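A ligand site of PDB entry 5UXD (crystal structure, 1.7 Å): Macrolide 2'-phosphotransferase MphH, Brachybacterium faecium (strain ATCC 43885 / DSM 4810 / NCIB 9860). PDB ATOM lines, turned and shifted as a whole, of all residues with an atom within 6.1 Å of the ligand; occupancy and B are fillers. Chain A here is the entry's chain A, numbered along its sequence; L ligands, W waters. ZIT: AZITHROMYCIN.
An oxygen (O4B) of the ligand lies close to the backbone carbonyl oxygen of Gly 273, at 3.3 Å. The backbone NH (N) of Tyr 274 sits at hydrogen-bond distance from an oxygen (O4B) of the ligand (3.3 Å).
Residues that only touch the ligand: Tyr 277 (3.5 Å), Ala 270 (3.5 Å), Phe 231 (3.5 Å), Glu 198 (3.6 Å) and Tyr 200 (3.9 Å). Hydrophobic or aromatic side chains that line the ligand: Phe 231, Ala 270, Tyr 274 and Tyr 277. Within 4 Å of the ligand: Glu 198, Tyr 200, Phe 231, Ala 270, Gly 273, Tyr 274 and Tyr 277. The nearest printed residue that does not touch the ligand is Phe 267 (4.5 Å).
Water W1 bridges the side-chain carboxylate (OE2) of Glu 198 (2.6 Å) and an oxygen (O2A) of the ligand (3.2 Å).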
ATOM      1  N   LEU A  33     -24.913  23.249 -27.236  1.00  0.00           N
ATOM      2  CA  LEU A  33     -25.648  23.164 -28.488  1.00  0.00           C
ATOM      3  C   LEU A  33     -26.809  22.179 -28.418  1.00  0.00           C
ATOM      4  O   LEU A  33     -27.766  22.304 -29.193  1.00  0.00           O
ATOM      5  CB  LEU A  33     -24.714  22.767 -29.628  1.00  0.00           C
ATOM      6  CG  LEU A  33     -23.610  23.752 -30.004  1.00  0.00           C
ATOM      7  CD1 LEU A  33     -22.680  23.115 -31.035  1.00  0.00           C
ATOM      8  CD2 LEU A  33     -24.194  25.055 -30.538  1.00  0.00           C
ATOM      9  N   LEU A 102      -9.888  20.640 -15.677  1.00  0.00           N
ATOM     10  CA  LEU A 102      -9.654  21.640 -16.698  1.00  0.00           C
ATOM     11  C   LEU A 102     -10.973  22.348 -16.956  1.00  0.00           C
ATOM     12  O   LEU A 102     -11.990  21.696 -17.195  1.00  0.00           O
ATOM     13  CB  LEU A 102      -9.126  20.979 -17.982  1.00  0.00           C
ATOM     14  CG  LEU A 102      -8.732  21.795 -19.222  1.00  0.00           C
ATOM     15  CD1 LEU A 102      -7.747  21.005 -20.061  1.00  0.00           C
ATOM     16  CD2 LEU A 102      -9.942  22.174 -20.069  1.00  0.00           C
ATOM     17  N   VAL A 104     -12.904  25.728 -19.122  1.00  0.00           N
ATOM     18  CA  VAL A 104     -12.814  26.661 -20.256  1.00  0.00           C
ATOM     19  C   VAL A 104     -13.774  27.806 -19.988  1.00  0.00           C
ATOM     20  O   VAL A 104     -14.975  27.576 -19.771  1.00  0.00           O
ATOM     21  CB  VAL A 104     -13.134  25.968 -21.587  1.00  0.00           C
ATOM     22  CG1 VAL A 104     -13.204  26.999 -22.721  1.00  0.00           C
ATOM     23  CG2 VAL A 104     -12.116  24.893 -21.900  1.00  0.00           C
ATOM     24  N   VAL A 110      -8.657  28.426 -21.503  1.00  0.00           N
ATOM     25  CA  VAL A 110      -8.551  27.122 -20.858  1.00  0.00           C
ATOM     26  C   VAL A 110      -7.684  27.274 -19.618  1.00  0.00           C
ATOM     27  O   VAL A 110      -6.630  27.926 -19.667  1.00  0.00           O
ATOM     28  CB  VAL A 110      -8.002  26.056 -21.820  1.00  0.00           C
ATOM     29  CG1 VAL A 110      -8.928  25.881 -23.019  1.00  0.00           C
ATOM     30  CG2 VAL A 110      -6.597  26.407 -22.296  1.00  0.00           C
ATOM     31  N   TRP A 112      -5.970  24.989 -16.401  1.00  0.00           N
ATOM     32  CA  TRP A 112      -5.688  23.656 -15.891  1.00  0.00           C
ATOM     33  C   TRP A 112      -5.647  23.663 -14.368  1.00  0.00           C
ATOM     34  O   TRP A 112      -5.086  24.576 -13.748  1.00  0.00           O
ATOM     35  CB  TRP A 112      -4.364  23.133 -16.439  1.00  0.00           C
ATOM     36  CG  TRP A 112      -4.403  22.812 -17.901  1.00  0.00           C
ATOM     37  CD1 TRP A 112      -4.354  23.700 -18.931  1.00  0.00           C
ATOM     38  CD2 TRP A 112      -4.535  21.513 -18.490  1.00  0.00           C
ATOM     39  NE1 TRP A 112      -4.433  23.028 -20.136  1.00  0.00           N
ATOM     40  CE2 TRP A 112      -4.545  21.690 -19.891  1.00  0.00           C
ATOM     41  CE3 TRP A 112      -4.639  20.221 -17.971  1.00  0.00           C
ATOM     42  CZ2 TRP A 112      -4.647  20.620 -20.774  1.00  0.00           C
ATOM     43  CZ3 TRP A 112      -4.746  19.159 -18.852  1.00  0.00           C
ATOM     44  CH2 TRP A 112      -4.752  19.362 -20.242  1.00  0.00           C
ATOM     45  N   GLU A 198     -13.005  10.021 -24.360  1.00  0.00           N
ATOM     46  CA  GLU A 198     -12.554  11.406 -24.307  1.00  0.00           C
ATOM     47  C   GLU A 198     -12.064  11.701 -22.896  1.00  0.00           C
ATOM     48  O   GLU A 198     -12.452  12.685 -22.248  1.00  0.00           O
ATOM     49  CB  GLU A 198     -13.670  12.344 -24.751  1.00  0.00           C
ATOM     50  CG  GLU A 198     -13.251  13.291 -25.869  1.00  0.00           C
ATOM     51  CD  GLU A 198     -14.412  14.022 -26.503  1.00  0.00           C
ATOM     52  OE1 GLU A 198     -14.856  13.610 -27.600  1.00  0.00           O
ATOM     53  OE2 GLU A 198     -14.890  15.001 -25.895  1.00  0.00           O
ATOM     54  N   TYR A 200      -9.826  13.118 -20.861  1.00  0.00           N
ATOM     55  CA  TYR A 200      -8.851  14.145 -20.550  1.00  0.00           C
ATOM     56  C   TYR A 200      -9.414  14.989 -19.408  1.00  0.00           C
ATOM     57  O   TYR A 200     -10.581  14.830 -19.044  1.00  0.00           O
ATOM     58  CB  TYR A 200      -8.503  14.980 -21.798  1.00  0.00           C
ATOM     59  CG  TYR A 200      -9.611  15.751 -22.456  1.00  0.00           C
ATOM     60  CD1 TYR A 200     -10.497  15.135 -23.330  1.00  0.00           C
ATOM     61  CD2 TYR A 200      -9.734  17.126 -22.270  1.00  0.00           C
ATOM     62  CE1 TYR A 200     -11.502  15.837 -23.961  1.00  0.00           C
ATOM     63  CE2 TYR A 200     -10.729  17.846 -22.891  1.00  0.00           C
ATOM     64  CZ  TYR A 200     -11.615  17.200 -23.732  1.00  0.00           C
ATOM     65  OH  TYR A 200     -12.609  17.911 -24.368  1.00  0.00           O
ATOM     66  N   THR A 219     -19.433   9.549 -25.504  1.00  0.00           N
ATOM     67  CA  THR A 219     -18.505   8.975 -26.479  1.00  0.00           C
ATOM     68  C   THR A 219     -18.147   7.518 -26.169  1.00  0.00           C
ATOM     69  O   THR A 219     -17.291   6.947 -26.865  1.00  0.00           O
ATOM     70  CB  THR A 219     -17.223   9.813 -26.567  1.00  0.00           C
ATOM     71  OG1 THR A 219     -16.657  10.006 -25.259  1.00  0.00           O
ATOM     72  CG2 THR A 219     -17.515  11.179 -27.168  1.00  0.00           C
ATOM     73  N   PHE A 231      -4.764  10.625 -24.149  1.00  0.00           N
ATOM     74  CA  PHE A 231      -4.620  12.033 -23.803  1.00  0.00           C
ATOM     75  C   PHE A 231      -3.548  12.232 -22.740  1.00  0.00           C
ATOM     76  O   PHE A 231      -2.788  13.209 -22.790  1.00  0.00           O
ATOM     77  CB  PHE A 231      -5.976  12.626 -23.372  1.00  0.00           C
ATOM     78  CG  PHE A 231      -7.050  12.500 -24.442  1.00  0.00           C
ATOM     79  CD1 PHE A 231      -6.996  13.288 -25.586  1.00  0.00           C
ATOM     80  CD2 PHE A 231      -8.076  11.566 -24.346  1.00  0.00           C
ATOM     81  CE1 PHE A 231      -7.957  13.167 -26.587  1.00  0.00           C
ATOM     82  CE2 PHE A 231      -9.034  11.434 -25.339  1.00  0.00           C
ATOM     83  CZ  PHE A 231      -8.972  12.236 -26.464  1.00  0.00           C
ATOM     84  N   PHE A 267      -3.426  10.282 -31.900  1.00  0.00           N
ATOM     85  CA  PHE A 267      -3.709  11.691 -31.617  1.00  0.00           C
ATOM     86  C   PHE A 267      -3.420  12.543 -32.843  1.00  0.00           C
ATOM     87  O   PHE A 267      -4.138  13.505 -33.124  1.00  0.00           O
ATOM     88  CB  PHE A 267      -2.880  12.142 -30.422  1.00  0.00           C
ATOM     89  CG  PHE A 267      -3.259  13.478 -29.874  1.00  0.00           C
ATOM     90  CD1 PHE A 267      -4.263  13.592 -28.937  1.00  0.00           C
ATOM     91  CD2 PHE A 267      -2.586  14.614 -30.279  1.00  0.00           C
ATOM     92  CE1 PHE A 267      -4.623  14.836 -28.418  1.00  0.00           C
ATOM     93  CE2 PHE A 267      -2.930  15.867 -29.751  1.00  0.00           C
ATOM     94  CZ  PHE A 267      -3.944  15.963 -28.825  1.00  0.00           C
ATOM     95  N   ALA A 270      -6.251  13.085 -35.505  1.00  0.00           N
ATOM     96  CA  ALA A 270      -7.413  13.932 -35.220  1.00  0.00           C
ATOM     97  C   ALA A 270      -7.989  14.611 -36.450  1.00  0.00           C
ATOM     98  O   ALA A 270      -9.216  14.749 -36.504  1.00  0.00           O
ATOM     99  CB  ALA A 270      -7.036  14.976 -34.152  1.00  0.00           C
ATOM    100  N   PRO A 271      -7.208  15.086 -37.435  1.00  0.00           N
ATOM    101  CA  PRO A 271      -7.846  15.678 -38.616  1.00  0.00           C
ATOM    102  C   PRO A 271      -8.806  14.739 -39.323  1.00  0.00           C
ATOM    103  O   PRO A 271      -9.769  15.213 -39.947  1.00  0.00           O
ATOM    104  CB  PRO A 271      -6.660  16.060 -39.513  1.00  0.00           C
ATOM    105  CG  PRO A 271      -5.532  16.317 -38.499  1.00  0.00           C
ATOM    106  CD  PRO A 271      -5.738  15.261 -37.468  1.00  0.00           C
ATOM    107  N   LEU A 272      -8.579  13.417 -39.257  1.00  0.00           N
ATOM    108  CA  LEU A 272      -9.558  12.521 -39.853  1.00  0.00           C
ATOM    109  C   LEU A 272     -10.864  12.527 -39.071  1.00  0.00           C
ATOM    110  O   LEU A 272     -11.953  12.469 -39.654  1.00  0.00           O
ATOM    111  CB  LEU A 272      -9.029  11.099 -39.934  1.00  0.00           C
ATOM    112  CG  LEU A 272      -7.884  10.808 -40.915  1.00  0.00           C
ATOM    113  CD1 LEU A 272      -7.353   9.369 -40.735  1.00  0.00           C
ATOM    114  CD2 LEU A 272      -8.326  11.075 -42.347  1.00  0.00           C
ATOM    115  N   GLY A 273     -10.818  12.656 -37.745  1.00  0.00           N
ATOM    116  CA  GLY A 273     -12.059  12.834 -36.989  1.00  0.00           C
ATOM    117  C   GLY A 273     -12.801  14.093 -37.389  1.00  0.00           C
ATOM    118  O   GLY A 273     -14.043  14.102 -37.462  1.00  0.00           O
ATOM    119  N   TYR A 274     -12.073  15.190 -37.637  1.00  0.00           N
ATOM    120  CA  TYR A 274     -12.709  16.415 -38.128  1.00  0.00           C
ATOM    121  C   TYR A 274     -13.367  16.179 -39.479  1.00  0.00           C
ATOM    122  O   TYR A 274     -14.477  16.663 -39.735  1.00  0.00           O
ATOM    123  CB  TYR A 274     -11.663  17.533 -38.227  1.00  0.00           C
ATOM    124  CG  TYR A 274     -12.103  18.879 -37.694  1.00  0.00           C
ATOM    125  CD1 TYR A 274     -13.385  19.362 -37.913  1.00  0.00           C
ATOM    126  CD2 TYR A 274     -11.217  19.681 -36.983  1.00  0.00           C
ATOM    127  CE1 TYR A 274     -13.779  20.598 -37.417  1.00  0.00           C
ATOM    128  CE2 TYR A 274     -11.604  20.923 -36.484  1.00  0.00           C
ATOM    129  CZ  TYR A 274     -12.892  21.377 -36.705  1.00  0.00           C
ATOM    130  OH  TYR A 274     -13.286  22.613 -36.209  1.00  0.00           O
ATOM    131  N   GLY A 275     -12.677  15.466 -40.378  1.00  0.00           N
ATOM    132  CA  GLY A 275     -13.262  15.175 -41.684  1.00  0.00           C
ATOM    133  C   GLY A 275     -14.536  14.373 -41.557  1.00  0.00           C
ATOM    134  O   GLY A 275     -15.552  14.680 -42.205  1.00  0.00           O
ATOM    135  N   TYR A 277     -16.577  14.238 -38.965  1.00  0.00           N
ATOM    136  CA  TYR A 277     -17.605  15.106 -38.399  1.00  0.00           C
ATOM    137  C   TYR A 277     -18.215  15.994 -39.484  1.00  0.00           C
ATOM    138  O   TYR A 277     -19.440  16.094 -39.596  1.00  0.00           O
ATOM    139  CB  TYR A 277     -17.018  15.952 -37.264  1.00  0.00           C
ATOM    140  CG  TYR A 277     -18.022  16.834 -36.541  1.00  0.00           C
ATOM    141  CD1 TYR A 277     -17.864  18.218 -36.511  1.00  0.00           C
ATOM    142  CD2 TYR A 277     -19.122  16.286 -35.913  1.00  0.00           C
ATOM    143  CE1 TYR A 277     -18.777  19.026 -35.854  1.00  0.00           C
ATOM    144  CE2 TYR A 277     -20.051  17.094 -35.250  1.00  0.00           C
ATOM    145  CZ  TYR A 277     -19.874  18.457 -35.233  1.00  0.00           C
ATOM    146  OH  TYR A 277     -20.786  19.256 -34.591  1.00  0.00           O
HETATM  147  C1  ZIT L   1      -9.009  17.752 -27.851  1.00  0.00           C
HETATM  148  C2  ZIT L   1     -10.361  17.013 -28.135  1.00  0.00           C
HETATM  149  C3  ZIT L   1     -10.793  17.483 -29.499  1.00  0.00           C
HETATM  150  C4  ZIT L   1     -11.799  18.632 -29.221  1.00  0.00           C
HETATM  151  C5  ZIT L   1     -12.385  19.219 -30.522  1.00  0.00           C
HETATM  152  C6  ZIT L   1     -11.801  20.591 -30.734  1.00  0.00           C
HETATM  153  C7  ZIT L   1     -12.552  21.650 -29.891  1.00  0.00           C
HETATM  154  C8  ZIT L   1     -11.920  23.061 -30.140  1.00  0.00           C
HETATM  155  C9  ZIT L   1     -11.089  23.520 -28.909  1.00  0.00           C
HETATM  156  N10 ZIT L   1      -9.669  22.881 -28.949  1.00  0.00           N
HETATM  157  C11 ZIT L   1      -9.093  22.665 -27.636  1.00  0.00           C
HETATM  158  C12 ZIT L   1      -8.308  21.343 -27.635  1.00  0.00           C
HETATM  159  C13 ZIT L   1      -7.933  20.773 -26.269  1.00  0.00           C
HETATM  160  C14 ZIT L   1      -7.655  19.278 -26.419  1.00  0.00           C
HETATM  161  C15 ZIT L   1      -6.969  18.755 -25.164  1.00  0.00           C
HETATM  162  C16 ZIT L   1      -6.894  17.200 -25.198  1.00  0.00           C
HETATM  163  C17 ZIT L   1     -10.190  15.537 -27.956  1.00  0.00           C
HETATM  164  C18 ZIT L   1     -12.865  18.142 -28.285  1.00  0.00           C
HETATM  165  C19 ZIT L   1     -11.881  20.943 -32.224  1.00  0.00           C
HETATM  166  C20 ZIT L   1     -12.974  24.015 -30.426  1.00  0.00           C
HETATM  167  C21 ZIT L   1      -8.798  23.658 -29.838  1.00  0.00           C
HETATM  168  C22 ZIT L   1      -8.208  23.821 -27.226  1.00  0.00           C
HETATM  169  C23 ZIT L   1      -9.047  20.967 -25.237  1.00  0.00           C
HETATM  170  O1  ZIT L   1      -8.103  17.709 -28.657  1.00  0.00           O
HETATM  171  O6  ZIT L   1     -10.436  20.613 -30.346  1.00  0.00           O
HETATM  172  O12 ZIT L   1      -7.129  21.466 -28.396  1.00  0.00           O
HETATM  173  O13 ZIT L   1      -6.723  21.422 -25.806  1.00  0.00           O
HETATM  174  O14 ZIT L   1      -8.894  18.558 -26.574  1.00  0.00           O
HETATM  175  C1A ZIT L   1     -14.530  18.415 -31.237  1.00  0.00           C
HETATM  176  C2A ZIT L   1     -16.001  18.419 -30.893  1.00  0.00           C
HETATM  177  C3A ZIT L   1     -16.689  17.343 -31.646  1.00  0.00           C
HETATM  178  C4A ZIT L   1     -16.446  17.480 -33.096  1.00  0.00           C
HETATM  179  C5A ZIT L   1     -14.981  17.720 -33.462  1.00  0.00           C
HETATM  180  C6A ZIT L   1     -14.823  18.134 -34.868  1.00  0.00           C
HETATM  181  C7A ZIT L   1     -18.768  18.570 -31.819  1.00  0.00           C
HETATM  182  C8A ZIT L   1     -18.852  16.207 -31.902  1.00  0.00           C
HETATM  183  O1A ZIT L   1     -13.803  19.313 -30.429  1.00  0.00           O
HETATM  184  O2A ZIT L   1     -16.208  18.241 -29.492  1.00  0.00           O
HETATM  185  N3A ZIT L   1     -18.155  17.369 -31.336  1.00  0.00           N
HETATM  186  O5A ZIT L   1     -14.338  18.756 -32.649  1.00  0.00           O
HETATM  187  C1B ZIT L   1     -10.399  15.837 -31.212  1.00  0.00           C
HETATM  188  C2B ZIT L   1     -10.760  14.382 -31.430  1.00  0.00           C
HETATM  189  C3B ZIT L   1     -11.880  14.195 -32.392  1.00  0.00           C
HETATM  190  C4B ZIT L   1     -11.617  14.925 -33.650  1.00  0.00           C
HETATM  191  C5B ZIT L   1     -11.385  16.381 -33.382  1.00  0.00           C
HETATM  192  C6B ZIT L   1     -11.165  17.067 -34.701  1.00  0.00           C
HETATM  193  C7B ZIT L   1     -12.043  12.654 -32.671  1.00  0.00           C
HETATM  194  C8B ZIT L   1     -13.864  13.899 -31.018  1.00  0.00           C
HETATM  195  O1B ZIT L   1     -11.350  16.438 -30.345  1.00  0.00           O
HETATM  196  O3B ZIT L   1     -13.092  14.754 -31.830  1.00  0.00           O
HETATM  197  O4B ZIT L   1     -12.801  14.880 -34.479  1.00  0.00           O
HETATM  198  O5B ZIT L   1     -10.253  16.634 -32.469  1.00  0.00           O
HETATM  199  O   HOH W   1     -16.053  17.190 -26.498  1.00  0.00           O
HETATM  200  O   HOH W   2     -18.927  17.278 -28.587  1.00  0.00           O
HETATM  201  O   HOH W   3     -16.827  13.973 -29.558  1.00  0.00           O
HETATM  202  O   HOH W   4      -4.050  15.507 -24.302  1.00  0.00           O
HETATM  203  O   HOH W   5     -12.305  21.658 -25.910  1.00  0.00           O
HETATM  204  O   HOH W   6      -7.234  14.962 -30.247  1.00  0.00           O
HETATM  205  O   HOH W   7     -15.609  21.160 -28.148  1.00  0.00           O
HETATM  206  O   HOH W   8      -8.183  18.196 -33.103  1.00  0.00           O
HETATM  207  O   HOH W   9     -15.839  14.453 -33.550  1.00  0.00           O
HETATM  208  O   HOH W  10     -14.991  11.423 -29.540  1.00  0.00           O
HETATM  209  O   HOH W  11      -5.343  19.393 -29.847  1.00  0.00           O
HETATM  210  O   HOH W  12      -8.278  20.807 -32.227  1.00  0.00           O
HETATM  211  O   HOH W  13      -5.365  23.189 -28.897  1.00  0.00           O
HETATM  212  O   HOH W  14     -11.739  21.169 -23.292  1.00  0.00           O
